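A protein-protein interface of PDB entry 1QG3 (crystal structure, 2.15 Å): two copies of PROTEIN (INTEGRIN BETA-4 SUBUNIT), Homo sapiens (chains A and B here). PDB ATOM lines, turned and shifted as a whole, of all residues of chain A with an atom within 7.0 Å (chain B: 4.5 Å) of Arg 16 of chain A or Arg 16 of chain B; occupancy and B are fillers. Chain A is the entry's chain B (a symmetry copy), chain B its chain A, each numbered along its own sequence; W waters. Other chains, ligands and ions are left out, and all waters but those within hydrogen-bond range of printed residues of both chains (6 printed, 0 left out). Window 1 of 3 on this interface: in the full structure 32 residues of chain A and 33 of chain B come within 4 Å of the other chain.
The guanidinium group of Arg 16 of chain B lies within hydrogen-bond range of the side-chain amide oxygen of Asn 60 of chain A (2.6 Å).
OD1 of Asn 60 of chain B lies within hydrogen-bond range of NH2 of Arg 16 of chain A.
The side-chain amide nitrogen (ND2) of Asn 60 of chain B is in hydrogen-bond range of the backbone carbonyl oxygen (O) of Val 94 of chain A (2.9 Å).
The backbone NH (N) of Asn 60 of chain A sits at hydrogen-bond distance from the backbone carbonyl oxygen (O) of Arg 16 of chain A (3.5 Å).
The backbone carbonyl oxygen (O) of Arg 16 of chain A is in hydrogen-bond range of the backbone NH (N) of Leu 61 of chain A (3.2 Å).
The backbone NH (N) of Leu 61 of chain B lies within hydrogen-bond range of the backbone carbonyl oxygen (O) of Arg 16 of chain B.
The backbone carbonyl oxygen of Asn 122 of chain A lies within hydrogen-bond range of the backbone NH of Glu 93 of chain A, 3.1 Å away.
The side-chain hydroxyl (OG) of Ser 15 of chain A sits at hydrogen-bond distance from the side-chain carboxylate (OE2) of Glu 93 of chain A, at 2.8 Å.
OG of Ser 15 of chain B lies within hydrogen-bond range of OE1 of Glu 93 of chain B (3.4 Å).
Among the printed residues, pairs that only touch across the chains: Ser 15 of chain A with Lys 17 of chain B (3.7 Å), Arg 16 of chain A with Arg 16 of chain B (3.8 Å), Lys 17 of chain A with Ser 15 of chain B (3.5 Å), Asn 60 of chain A with Glu 93 of chain B (2.8 Å), Glu 93 of chain A with Asn 60 of chain B (3.4 Å), Val 94 of chain A with Thr 59 of chain B (3.3 Å) and Asn 122 of chain A with Asn 60 of chain B (3.6 Å).
Printed residues of chain B within 4 Å of Ser 15 of chain A: Lys 17 (3.7 Å).
Arg 16 of chain A touches just these residues of chain B: Arg 16 and Asn 60.
Printed residues of chain B within 4 Å of Glu 93 of chain A: Asn 60 (3.4 Å).
Arg 16 of chain B touches two residues of chain A.
Of the printed residues of chain A, Lys 17 of chain B touches Ser 15.
The nearest printed residue of chain B that does not touch Arg 16 of chain A is Ser 15 of chain B (5.3 Å).
The nearest printed residue of chain A that does not touch Glu 93 of chain B is Thr 59 of chain A (4.3 Å).
Printed residues of chain A that touch a printed residue of chain B: Ser 15, Arg 16, Lys 17, Asn 60, Glu 93, Val 94 and Asn 122.
Printed residues of chain B that touch a printed residue of chain A: Ser 15, Arg 16, Lys 17, Thr 59, Asn 60 and Glu 93.
Among the printed residues, no Asp or Glu carboxylate lies within 4 Å of a Lys or Arg side-chain nitrogen of the other chain.
Ser 15 of chain A touches Lys 17 of chain B, and with the chains exchanged Lys 17 of chain A touches Ser 15 of chain B.
Arg 16 of chain B touches its own counterpart, Arg 16 of chain A.
Arg 16 of chain A touches Asn 60 of chain B, and with the chains exchanged Asn 60 of chain A touches Arg 16 of chain B.
Asn 60 of chain A touches Glu 93 of chain B, and with the chains exchanged Glu 93 of chain A touches Asn 60 of chain B.
10 positions are printed for both chains.
Of the 10 pairs that touch across the chains among the printed residues, 7 have their exchanged pair printed and touching as well.
Water W3 lies within hydrogen-bond range of the side-chain carboxylate (OE2) of Glu 93 of chain B, the side-chain amino group (NZ) of Lys 17 of chain A and the side-chain hydroxyl (OG) of Ser 15 of chain B.
Water W2 lies within hydrogen-bond range of the side-chain carboxylate (OE1) of Glu 93 of chain A, the side-chain amino group (NZ) of Lys 17 of chain B and the side-chain hydroxyl (OG) of Ser 15 of chain A.
Water W1 bridges the side-chain carboxylate (OE2) of Glu 93 of chain B (2.8 Å) and the side-chain hydroxyl (OG1) of Thr 59 of chain A (2.8 Å).
Water W6 lies within hydrogen-bond range of the side-chain hydroxyl of Thr 59 of chain B (2.8 Å), the backbone NH of Val 94 of chain A (2.9 Å) and the side-chain carboxylate of Glu 93 of chain A (2.9 Å).
Water W4 lies within hydrogen-bond range of N of Asn 60 of chain A (2.9 Å), O of Arg 16 of chain A (3.0 Å) and NH1 of Arg 16 of chain B (3.5 Å).
Water W5 lies within hydrogen-bond range of the backbone NH of Asn 60 of chain B, the guanidinium group of Arg 16 of chain A and the backbone carbonyl oxygen of Arg 16 of chain B.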
ATOM      1  N   ALA A  13      -1.490  18.403  11.973  1.00  0.00           N
ATOM      2  CA  ALA A  13      -1.364  19.787  12.423  1.00  0.00           C
ATOM      3  C   ALA A  13       0.053  20.076  12.882  1.00  0.00           C
ATOM      4  O   ALA A  13       0.429  19.764  14.010  1.00  0.00           O
ATOM      5  CB  ALA A  13      -2.344  20.068  13.554  1.00  0.00           C
ATOM      6  N   GLY A  14       0.840  20.677  11.999  1.00  0.00           N
ATOM      7  CA  GLY A  14       2.211  20.987  12.345  1.00  0.00           C
ATOM      8  C   GLY A  14       3.107  19.772  12.207  1.00  0.00           C
ATOM      9  O   GLY A  14       2.716  18.762  11.612  1.00  0.00           O
ATOM     10  N   SER A  15       4.303  19.874  12.777  1.00  0.00           N
ATOM     11  CA  SER A  15       5.301  18.815  12.717  1.00  0.00           C
ATOM     12  C   SER A  15       5.086  17.692  13.717  1.00  0.00           C
ATOM     13  O   SER A  15       4.941  17.937  14.914  1.00  0.00           O
ATOM     14  CB  SER A  15       6.693  19.409  12.937  1.00  0.00           C
ATOM     15  OG  SER A  15       7.653  18.388  13.140  1.00  0.00           O
ATOM     16  N   ARG A  16       5.071  16.458  13.222  1.00  0.00           N
ATOM     17  CA  ARG A  16       4.899  15.301  14.095  1.00  0.00           C
ATOM     18  C   ARG A  16       3.677  15.440  15.000  1.00  0.00           C
ATOM     19  O   ARG A  16       3.711  15.026  16.153  1.00  0.00           O
ATOM     20  CB  ARG A  16       6.150  15.117  14.968  1.00  0.00           C
ATOM     21  CG  ARG A  16       7.433  14.766  14.207  1.00  0.00           C
ATOM     22  CD  ARG A  16       8.576  14.522  15.184  1.00  0.00           C
ATOM     23  NE  ARG A  16       9.747  13.909  14.556  1.00  0.00           N
ATOM     24  CZ  ARG A  16      10.596  14.550  13.761  1.00  0.00           C
ATOM     25  NH1 ARG A  16      10.413  15.835  13.488  1.00  0.00           N
ATOM     26  NH2 ARG A  16      11.634  13.900  13.244  1.00  0.00           N
ATOM     27  N   LYS A  17       2.603  16.025  14.482  1.00  0.00           N
ATOM     28  CA  LYS A  17       1.393  16.204  15.276  1.00  0.00           C
ATOM     29  C   LYS A  17       0.103  16.030  14.480  1.00  0.00           C
ATOM     30  O   LYS A  17       0.077  16.247  13.261  1.00  0.00           O
ATOM     31  CB  LYS A  17       1.376  17.590  15.925  1.00  0.00           C
ATOM     32  CG  LYS A  17       2.332  17.761  17.092  1.00  0.00           C
ATOM     33  CD  LYS A  17       2.136  19.121  17.745  1.00  0.00           C
ATOM     34  CE  LYS A  17       2.615  20.247  16.847  1.00  0.00           C
ATOM     35  NZ  LYS A  17       4.088  20.131  16.585  1.00  0.00           N
ATOM     36  N   ILE A  18      -0.956  15.656  15.200  1.00  0.00           N
ATOM     37  CA  ILE A  18      -2.289  15.450  14.644  1.00  0.00           C
ATOM     38  C   ILE A  18      -3.340  16.048  15.589  1.00  0.00           C
ATOM     39  O   ILE A  18      -3.313  15.806  16.796  1.00  0.00           O
ATOM     40  CB  ILE A  18      -2.620  13.947  14.481  1.00  0.00           C
ATOM     41  CG1 ILE A  18      -1.805  13.340  13.340  1.00  0.00           C
ATOM     42  CG2 ILE A  18      -4.117  13.766  14.208  1.00  0.00           C
ATOM     43  CD1 ILE A  18      -1.989  11.843  13.224  1.00  0.00           C
ATOM     44  N   LEU A  58      -2.199  15.182  19.367  1.00  0.00           N
ATOM     45  CA  LEU A  58      -1.338  14.012  19.477  1.00  0.00           C
ATOM     46  C   LEU A  58       0.039  14.528  19.045  1.00  0.00           C
ATOM     47  O   LEU A  58       0.176  15.081  17.944  1.00  0.00           O
ATOM     48  CB  LEU A  58      -1.802  12.890  18.535  1.00  0.00           C
ATOM     49  CG  LEU A  58      -3.294  12.508  18.527  1.00  0.00           C
ATOM     50  CD1 LEU A  58      -3.504  11.294  17.615  1.00  0.00           C
ATOM     51  CD2 LEU A  58      -3.777  12.207  19.943  1.00  0.00           C
ATOM     52  N   THR A  59       1.044  14.363  19.909  1.00  0.00           N
ATOM     53  CA  THR A  59       2.401  14.825  19.612  1.00  0.00           C
ATOM     54  C   THR A  59       3.450  13.713  19.692  1.00  0.00           C
ATOM     55  O   THR A  59       3.148  12.586  20.074  1.00  0.00           O
ATOM     56  CB  THR A  59       2.826  15.959  20.569  1.00  0.00           C
ATOM     57  OG1 THR A  59       2.938  15.444  21.901  1.00  0.00           O
ATOM     58  CG2 THR A  59       1.789  17.078  20.564  1.00  0.00           C
ATOM     59  N   ASN A  60       4.690  14.050  19.338  1.00  0.00           N
ATOM     60  CA  ASN A  60       5.803  13.099  19.334  1.00  0.00           C
ATOM     61  C   ASN A  60       5.556  11.937  18.393  1.00  0.00           C
ATOM     62  O   ASN A  60       5.996  10.818  18.646  1.00  0.00           O
ATOM     63  CB  ASN A  60       6.076  12.565  20.739  1.00  0.00           C
ATOM     64  CG  ASN A  60       6.524  13.644  21.679  1.00  0.00           C
ATOM     65  OD1 ASN A  60       7.385  14.453  21.336  1.00  0.00           O
ATOM     66  ND2 ASN A  60       5.952  13.666  22.882  1.00  0.00           N
ATOM     67  N   LEU A  61       4.847  12.212  17.304  1.00  0.00           N
ATOM     68  CA  LEU A  61       4.543  11.195  16.313  1.00  0.00           C
ATOM     69  C   LEU A  61       5.686  11.070  15.304  1.00  0.00           C
ATOM     70  O   LEU A  61       6.600  11.901  15.268  1.00  0.00           O
ATOM     71  CB  LEU A  61       3.259  11.572  15.575  1.00  0.00           C
ATOM     72  CG  LEU A  61       2.074  11.917  16.482  1.00  0.00           C
ATOM     73  CD1 LEU A  61       0.862  12.283  15.640  1.00  0.00           C
ATOM     74  CD2 LEU A  61       1.767  10.741  17.385  1.00  0.00           C
ATOM     75  N   TYR A  62       5.641  10.021  14.492  1.00  0.00           N
ATOM     76  CA  TYR A  62       6.644   9.825  13.453  1.00  0.00           C
ATOM     77  C   TYR A  62       6.169  10.605  12.245  1.00  0.00           C
ATOM     78  O   TYR A  62       4.970  10.687  11.986  1.00  0.00           O
ATOM     79  CB  TYR A  62       6.754   8.362  13.040  1.00  0.00           C
ATOM     80  CG  TYR A  62       7.490   7.482  14.010  1.00  0.00           C
ATOM     81  CD1 TYR A  62       6.891   7.060  15.190  1.00  0.00           C
ATOM     82  CD2 TYR A  62       8.792   7.069  13.745  1.00  0.00           C
ATOM     83  CE1 TYR A  62       7.570   6.242  16.085  1.00  0.00           C
ATOM     84  CE2 TYR A  62       9.480   6.254  14.632  1.00  0.00           C
ATOM     85  CZ  TYR A  62       8.863   5.843  15.799  1.00  0.00           C
ATOM     86  OH  TYR A  62       9.540   5.027  16.675  1.00  0.00           O
ATOM     87  N   PRO A  63       7.100  11.198  11.488  1.00  0.00           N
ATOM     88  CA  PRO A  63       6.633  11.940  10.321  1.00  0.00           C
ATOM     89  C   PRO A  63       6.186  11.001   9.199  1.00  0.00           C
ATOM     90  O   PRO A  63       6.569   9.824   9.165  1.00  0.00           O
ATOM     91  CB  PRO A  63       7.841  12.803   9.948  1.00  0.00           C
ATOM     92  CG  PRO A  63       9.005  12.014  10.450  1.00  0.00           C
ATOM     93  CD  PRO A  63       8.521  11.467  11.767  1.00  0.00           C
ATOM     94  N   TYR A  64       5.352  11.526   8.306  1.00  0.00           N
ATOM     95  CA  TYR A  64       4.839  10.770   7.168  1.00  0.00           C
ATOM     96  C   TYR A  64       4.435   9.346   7.570  1.00  0.00           C
ATOM     97  O   TYR A  64       4.795   8.380   6.901  1.00  0.00           O
ATOM     98  CB  TYR A  64       5.901  10.729   6.063  1.00  0.00           C
ATOM     99  CG  TYR A  64       5.356  10.346   4.700  1.00  0.00           C
ATOM    100  CD1 TYR A  64       4.398  11.135   4.065  1.00  0.00           C
ATOM    101  CD2 TYR A  64       5.810   9.204   4.043  1.00  0.00           C
ATOM    102  CE1 TYR A  64       3.911  10.799   2.802  1.00  0.00           C
ATOM    103  CE2 TYR A  64       5.332   8.856   2.790  1.00  0.00           C
ATOM    104  CZ  TYR A  64       4.387   9.656   2.174  1.00  0.00           C
ATOM    105  OH  TYR A  64       3.931   9.312   0.920  1.00  0.00           O
ATOM    106  N   THR A  90       0.653  11.866   9.244  1.00  0.00           N
ATOM    107  CA  THR A  90       1.449  13.010   9.652  1.00  0.00           C
ATOM    108  C   THR A  90       2.197  13.600   8.455  1.00  0.00           C
ATOM    109  O   THR A  90       2.481  12.900   7.474  1.00  0.00           O
ATOM    110  CB  THR A  90       2.463  12.592  10.727  1.00  0.00           C
ATOM    111  OG1 THR A  90       3.301  11.550  10.216  1.00  0.00           O
ATOM    112  CG2 THR A  90       1.740  12.076  11.973  1.00  0.00           C
ATOM    113  N   HIS A  91       2.504  14.891   8.536  1.00  0.00           N
ATOM    114  CA  HIS A  91       3.235  15.569   7.471  1.00  0.00           C
ATOM    115  C   HIS A  91       4.636  14.995   7.342  1.00  0.00           C
ATOM    116  O   HIS A  91       5.107  14.267   8.216  1.00  0.00           O
ATOM    117  CB  HIS A  91       3.355  17.064   7.768  1.00  0.00           C
ATOM    118  CG  HIS A  91       2.063  17.809   7.671  1.00  0.00           C
ATOM    119  ND1 HIS A  91       1.240  17.733   6.569  1.00  0.00           N
ATOM    120  CD2 HIS A  91       1.466  18.675   8.527  1.00  0.00           C
ATOM    121  CE1 HIS A  91       0.193  18.517   6.748  1.00  0.00           C
ATOM    122  NE2 HIS A  91       0.305  19.102   7.927  1.00  0.00           N
ATOM    123  N   GLN A  92       5.300  15.328   6.242  1.00  0.00           N
ATOM    124  CA  GLN A  92       6.670  14.875   6.009  1.00  0.00           C
ATOM    125  C   GLN A  92       7.637  15.868   6.650  1.00  0.00           C
ATOM    126  O   GLN A  92       7.272  17.013   6.914  1.00  0.00           O
ATOM    127  CB  GLN A  92       6.978  14.833   4.512  1.00  0.00           C
ATOM    128  CG  GLN A  92       6.182  13.826   3.717  1.00  0.00           C
ATOM    129  CD  GLN A  92       6.496  13.906   2.240  1.00  0.00           C
ATOM    130  OE1 GLN A  92       7.658  13.818   1.837  1.00  0.00           O
ATOM    131  NE2 GLN A  92       5.462  14.079   1.422  1.00  0.00           N
ATOM    132  N   GLU A  93       8.863  15.410   6.895  1.00  0.00           N
ATOM    133  CA  GLU A  93       9.944  16.236   7.439  1.00  0.00           C
ATOM    134  C   GLU A  93      11.087  15.960   6.444  1.00  0.00           C
ATOM    135  O   GLU A  93      11.047  14.950   5.742  1.00  0.00           O
ATOM    136  CB  GLU A  93      10.361  15.768   8.846  1.00  0.00           C
ATOM    137  CG  GLU A  93       9.291  15.871   9.958  1.00  0.00           C
ATOM    138  CD  GLU A  93       8.807  17.298  10.208  1.00  0.00           C
ATOM    139  OE1 GLU A  93       9.624  18.240  10.094  1.00  0.00           O
ATOM    140  OE2 GLU A  93       7.611  17.476  10.538  1.00  0.00           O
ATOM    141  N   VAL A  94      12.091  16.829   6.358  1.00  0.00           N
ATOM    142  CA  VAL A  94      13.183  16.550   5.422  1.00  0.00           C
ATOM    143  C   VAL A  94      13.875  15.258   5.857  1.00  0.00           C
ATOM    144  O   VAL A  94      13.868  14.906   7.036  1.00  0.00           O
ATOM    145  CB  VAL A  94      14.214  17.707   5.362  1.00  0.00           C
ATOM    146  CG1 VAL A  94      13.547  18.970   4.789  1.00  0.00           C
ATOM    147  CG2 VAL A  94      14.791  17.975   6.742  1.00  0.00           C
ATOM    148  N   GLU A 120      16.432   7.812   7.921  1.00  0.00           N
ATOM    149  CA  GLU A 120      15.091   8.331   8.141  1.00  0.00           C
ATOM    150  C   GLU A 120      14.679   9.091   6.891  1.00  0.00           C
ATOM    151  O   GLU A 120      15.135  10.214   6.664  1.00  0.00           O
ATOM    152  CB  GLU A 120      15.050   9.282   9.341  1.00  0.00           C
ATOM    153  CG  GLU A 120      15.283   8.631  10.701  1.00  0.00           C
ATOM    154  CD  GLU A 120      16.735   8.666  11.139  1.00  0.00           C
ATOM    155  OE1 GLU A 120      17.338   9.761  11.105  1.00  0.00           O
ATOM    156  OE2 GLU A 120      17.270   7.601  11.530  1.00  0.00           O
ATOM    157  N   ASN A 122      11.620  10.024   6.299  1.00  0.00           N
ATOM    158  CA  ASN A 122      10.621  10.969   6.799  1.00  0.00           C
ATOM    159  C   ASN A 122       9.663  11.453   5.722  1.00  0.00           C
ATOM    160  O   ASN A 122       9.059  12.524   5.852  1.00  0.00           O
ATOM    161  CB  ASN A 122      11.302  12.181   7.440  1.00  0.00           C
ATOM    162  CG  ASN A 122      12.142  11.806   8.640  1.00  0.00           C
ATOM    163  OD1 ASN A 122      11.716  11.023   9.479  1.00  0.00           O
ATOM    164  ND2 ASN A 122      13.340  12.377   8.733  1.00  0.00           N
ATOM    165  N   GLY B  14       9.131  26.353  17.213  1.00  0.00           N
ATOM    166  CA  GLY B  14       8.274  25.214  16.968  1.00  0.00           C
ATOM    167  C   GLY B  14       8.828  23.948  17.588  1.00  0.00           C
ATOM    168  O   GLY B  14       9.760  23.989  18.394  1.00  0.00           O
ATOM    169  N   SER B  15       8.252  22.819  17.191  1.00  0.00           N
ATOM    170  CA  SER B  15       8.628  21.512  17.696  1.00  0.00           C
ATOM    171  C   SER B  15       9.896  20.947  17.088  1.00  0.00           C
ATOM    172  O   SER B  15      10.041  20.907  15.865  1.00  0.00           O
ATOM    173  CB  SER B  15       7.487  20.519  17.460  1.00  0.00           C
ATOM    174  OG  SER B  15       7.887  19.205  17.800  1.00  0.00           O
ATOM    175  N   ARG B  16      10.805  20.505  17.956  1.00  0.00           N
ATOM    176  CA  ARG B  16      12.068  19.902  17.538  1.00  0.00           C
ATOM    177  C   ARG B  16      12.857  20.687  16.483  1.00  0.00           C
ATOM    178  O   ARG B  16      13.453  20.102  15.582  1.00  0.00           O
ATOM    179  CB  ARG B  16      11.817  18.485  17.018  1.00  0.00           C
ATOM    180  CG  ARG B  16      11.326  17.474  18.057  1.00  0.00           C
ATOM    181  CD  ARG B  16      11.180  16.101  17.401  1.00  0.00           C
ATOM    182  NE  ARG B  16      10.826  15.028  18.322  1.00  0.00           N
ATOM    183  CZ  ARG B  16       9.665  14.927  18.969  1.00  0.00           C
ATOM    184  NH1 ARG B  16       8.716  15.844  18.807  1.00  0.00           N
ATOM    185  NH2 ARG B  16       9.447  13.896  19.778  1.00  0.00           N
ATOM    186  N   LYS B  17      12.847  22.009  16.565  1.00  0.00           N
ATOM    187  CA  LYS B  17      13.620  22.778  15.605  1.00  0.00           C
ATOM    188  C   LYS B  17      14.117  24.126  16.089  1.00  0.00           C
ATOM    189  O   LYS B  17      13.676  24.656  17.117  1.00  0.00           O
ATOM    190  CB  LYS B  17      12.874  22.938  14.276  1.00  0.00           C
ATOM    191  CG  LYS B  17      11.463  23.428  14.363  1.00  0.00           C
ATOM    192  CD  LYS B  17      10.872  23.572  12.960  1.00  0.00           C
ATOM    193  CE  LYS B  17       9.361  23.666  13.020  1.00  0.00           C
ATOM    194  NZ  LYS B  17       8.782  22.402  13.572  1.00  0.00           N
ATOM    195  N   LEU B  58      16.698  24.370  11.417  1.00  0.00           N
ATOM    196  CA  LEU B  58      17.340  23.106  11.736  1.00  0.00           C
ATOM    197  C   LEU B  58      16.201  22.212  12.219  1.00  0.00           C
ATOM    198  O   LEU B  58      15.509  22.548  13.190  1.00  0.00           O
ATOM    199  CB  LEU B  58      18.367  23.300  12.851  1.00  0.00           C
ATOM    200  CG  LEU B  58      19.415  24.415  12.684  1.00  0.00           C
ATOM    201  CD1 LEU B  58      20.435  24.311  13.814  1.00  0.00           C
ATOM    202  CD2 LEU B  58      20.113  24.296  11.329  1.00  0.00           C
ATOM    203  N   THR B  59      15.995  21.079  11.559  1.00  0.00           N
ATOM    204  CA  THR B  59      14.893  20.213  11.949  1.00  0.00           C
ATOM    205  C   THR B  59      15.288  18.803  12.375  1.00  0.00           C
ATOM    206  O   THR B  59      16.453  18.425  12.303  1.00  0.00           O
ATOM    207  CB  THR B  59      13.833  20.126  10.817  1.00  0.00           C
ATOM    208  OG1 THR B  59      14.317  19.291   9.755  1.00  0.00           O
ATOM    209  CG2 THR B  59      13.530  21.531  10.254  1.00  0.00           C
ATOM    210  N   ASN B  60      14.295  18.040  12.828  1.00  0.00           N
ATOM    211  CA  ASN B  60      14.493  16.667  13.288  1.00  0.00           C
ATOM    212  C   ASN B  60      15.489  16.601  14.443  1.00  0.00           C
ATOM    213  O   ASN B  60      16.294  15.670  14.547  1.00  0.00           O
ATOM    214  CB  ASN B  60      14.949  15.769  12.130  1.00  0.00           C
ATOM    215  CG  ASN B  60      13.886  15.631  11.045  1.00  0.00           C
ATOM    216  OD1 ASN B  60      12.697  15.464  11.342  1.00  0.00           O
ATOM    217  ND2 ASN B  60      14.308  15.695   9.781  1.00  0.00           N
ATOM    218  N   LEU B  61      15.419  17.595  15.321  1.00  0.00           N
ATOM    219  CA  LEU B  61      16.303  17.657  16.482  1.00  0.00           C
ATOM    220  C   LEU B  61      15.650  16.938  17.658  1.00  0.00           C
ATOM    221  O   LEU B  61      14.484  16.554  17.583  1.00  0.00           O
ATOM    222  CB  LEU B  61      16.552  19.119  16.871  1.00  0.00           C
ATOM    223  CG  LEU B  61      16.955  20.071  15.739  1.00  0.00           C
ATOM    224  CD1 LEU B  61      17.248  21.449  16.322  1.00  0.00           C
ATOM    225  CD2 LEU B  61      18.179  19.524  15.005  1.00  0.00           C
ATOM    226  N   PRO B  63      14.167  16.882  21.518  1.00  0.00           N
ATOM    227  CA  PRO B  63      13.474  17.902  22.312  1.00  0.00           C
ATOM    228  C   PRO B  63      14.304  18.221  23.562  1.00  0.00           C
ATOM    229  O   PRO B  63      15.091  17.388  24.011  1.00  0.00           O
ATOM    230  CB  PRO B  63      12.148  17.225  22.644  1.00  0.00           C
ATOM    231  CG  PRO B  63      12.569  15.799  22.840  1.00  0.00           C
ATOM    232  CD  PRO B  63      13.533  15.560  21.680  1.00  0.00           C
ATOM    233  N   GLU B  93       8.793  18.744  25.078  1.00  0.00           N
ATOM    234  CA  GLU B  93       7.707  18.012  24.446  1.00  0.00           C
ATOM    235  C   GLU B  93       7.185  17.135  25.588  1.00  0.00           C
ATOM    236  O   GLU B  93       7.957  16.766  26.475  1.00  0.00           O
ATOM    237  CB  GLU B  93       8.248  17.165  23.290  1.00  0.00           C
ATOM    238  CG  GLU B  93       7.356  17.127  22.058  1.00  0.00           C
ATOM    239  CD  GLU B  93       7.170  18.483  21.381  1.00  0.00           C
ATOM    240  OE1 GLU B  93       8.163  19.207  21.155  1.00  0.00           O
ATOM    241  OE2 GLU B  93       6.012  18.818  21.058  1.00  0.00           O
HETATM  242  O   HOH W   1       4.603  17.412  22.987  1.00  0.00           O
HETATM  243  O   HOH W   2       9.777  20.371  11.657  1.00  0.00           O
HETATM  244  O   HOH W   3       4.662  19.298  19.112  1.00  0.00           O
HETATM  245  O   HOH W   4       5.383  16.612  18.145  1.00  0.00           O
HETATM  246  O   HOH W   5      11.504  18.928  13.019  1.00  0.00           O
HETATM  247  O   HOH W   6      11.888  18.882   8.347  1.00  0.00           O
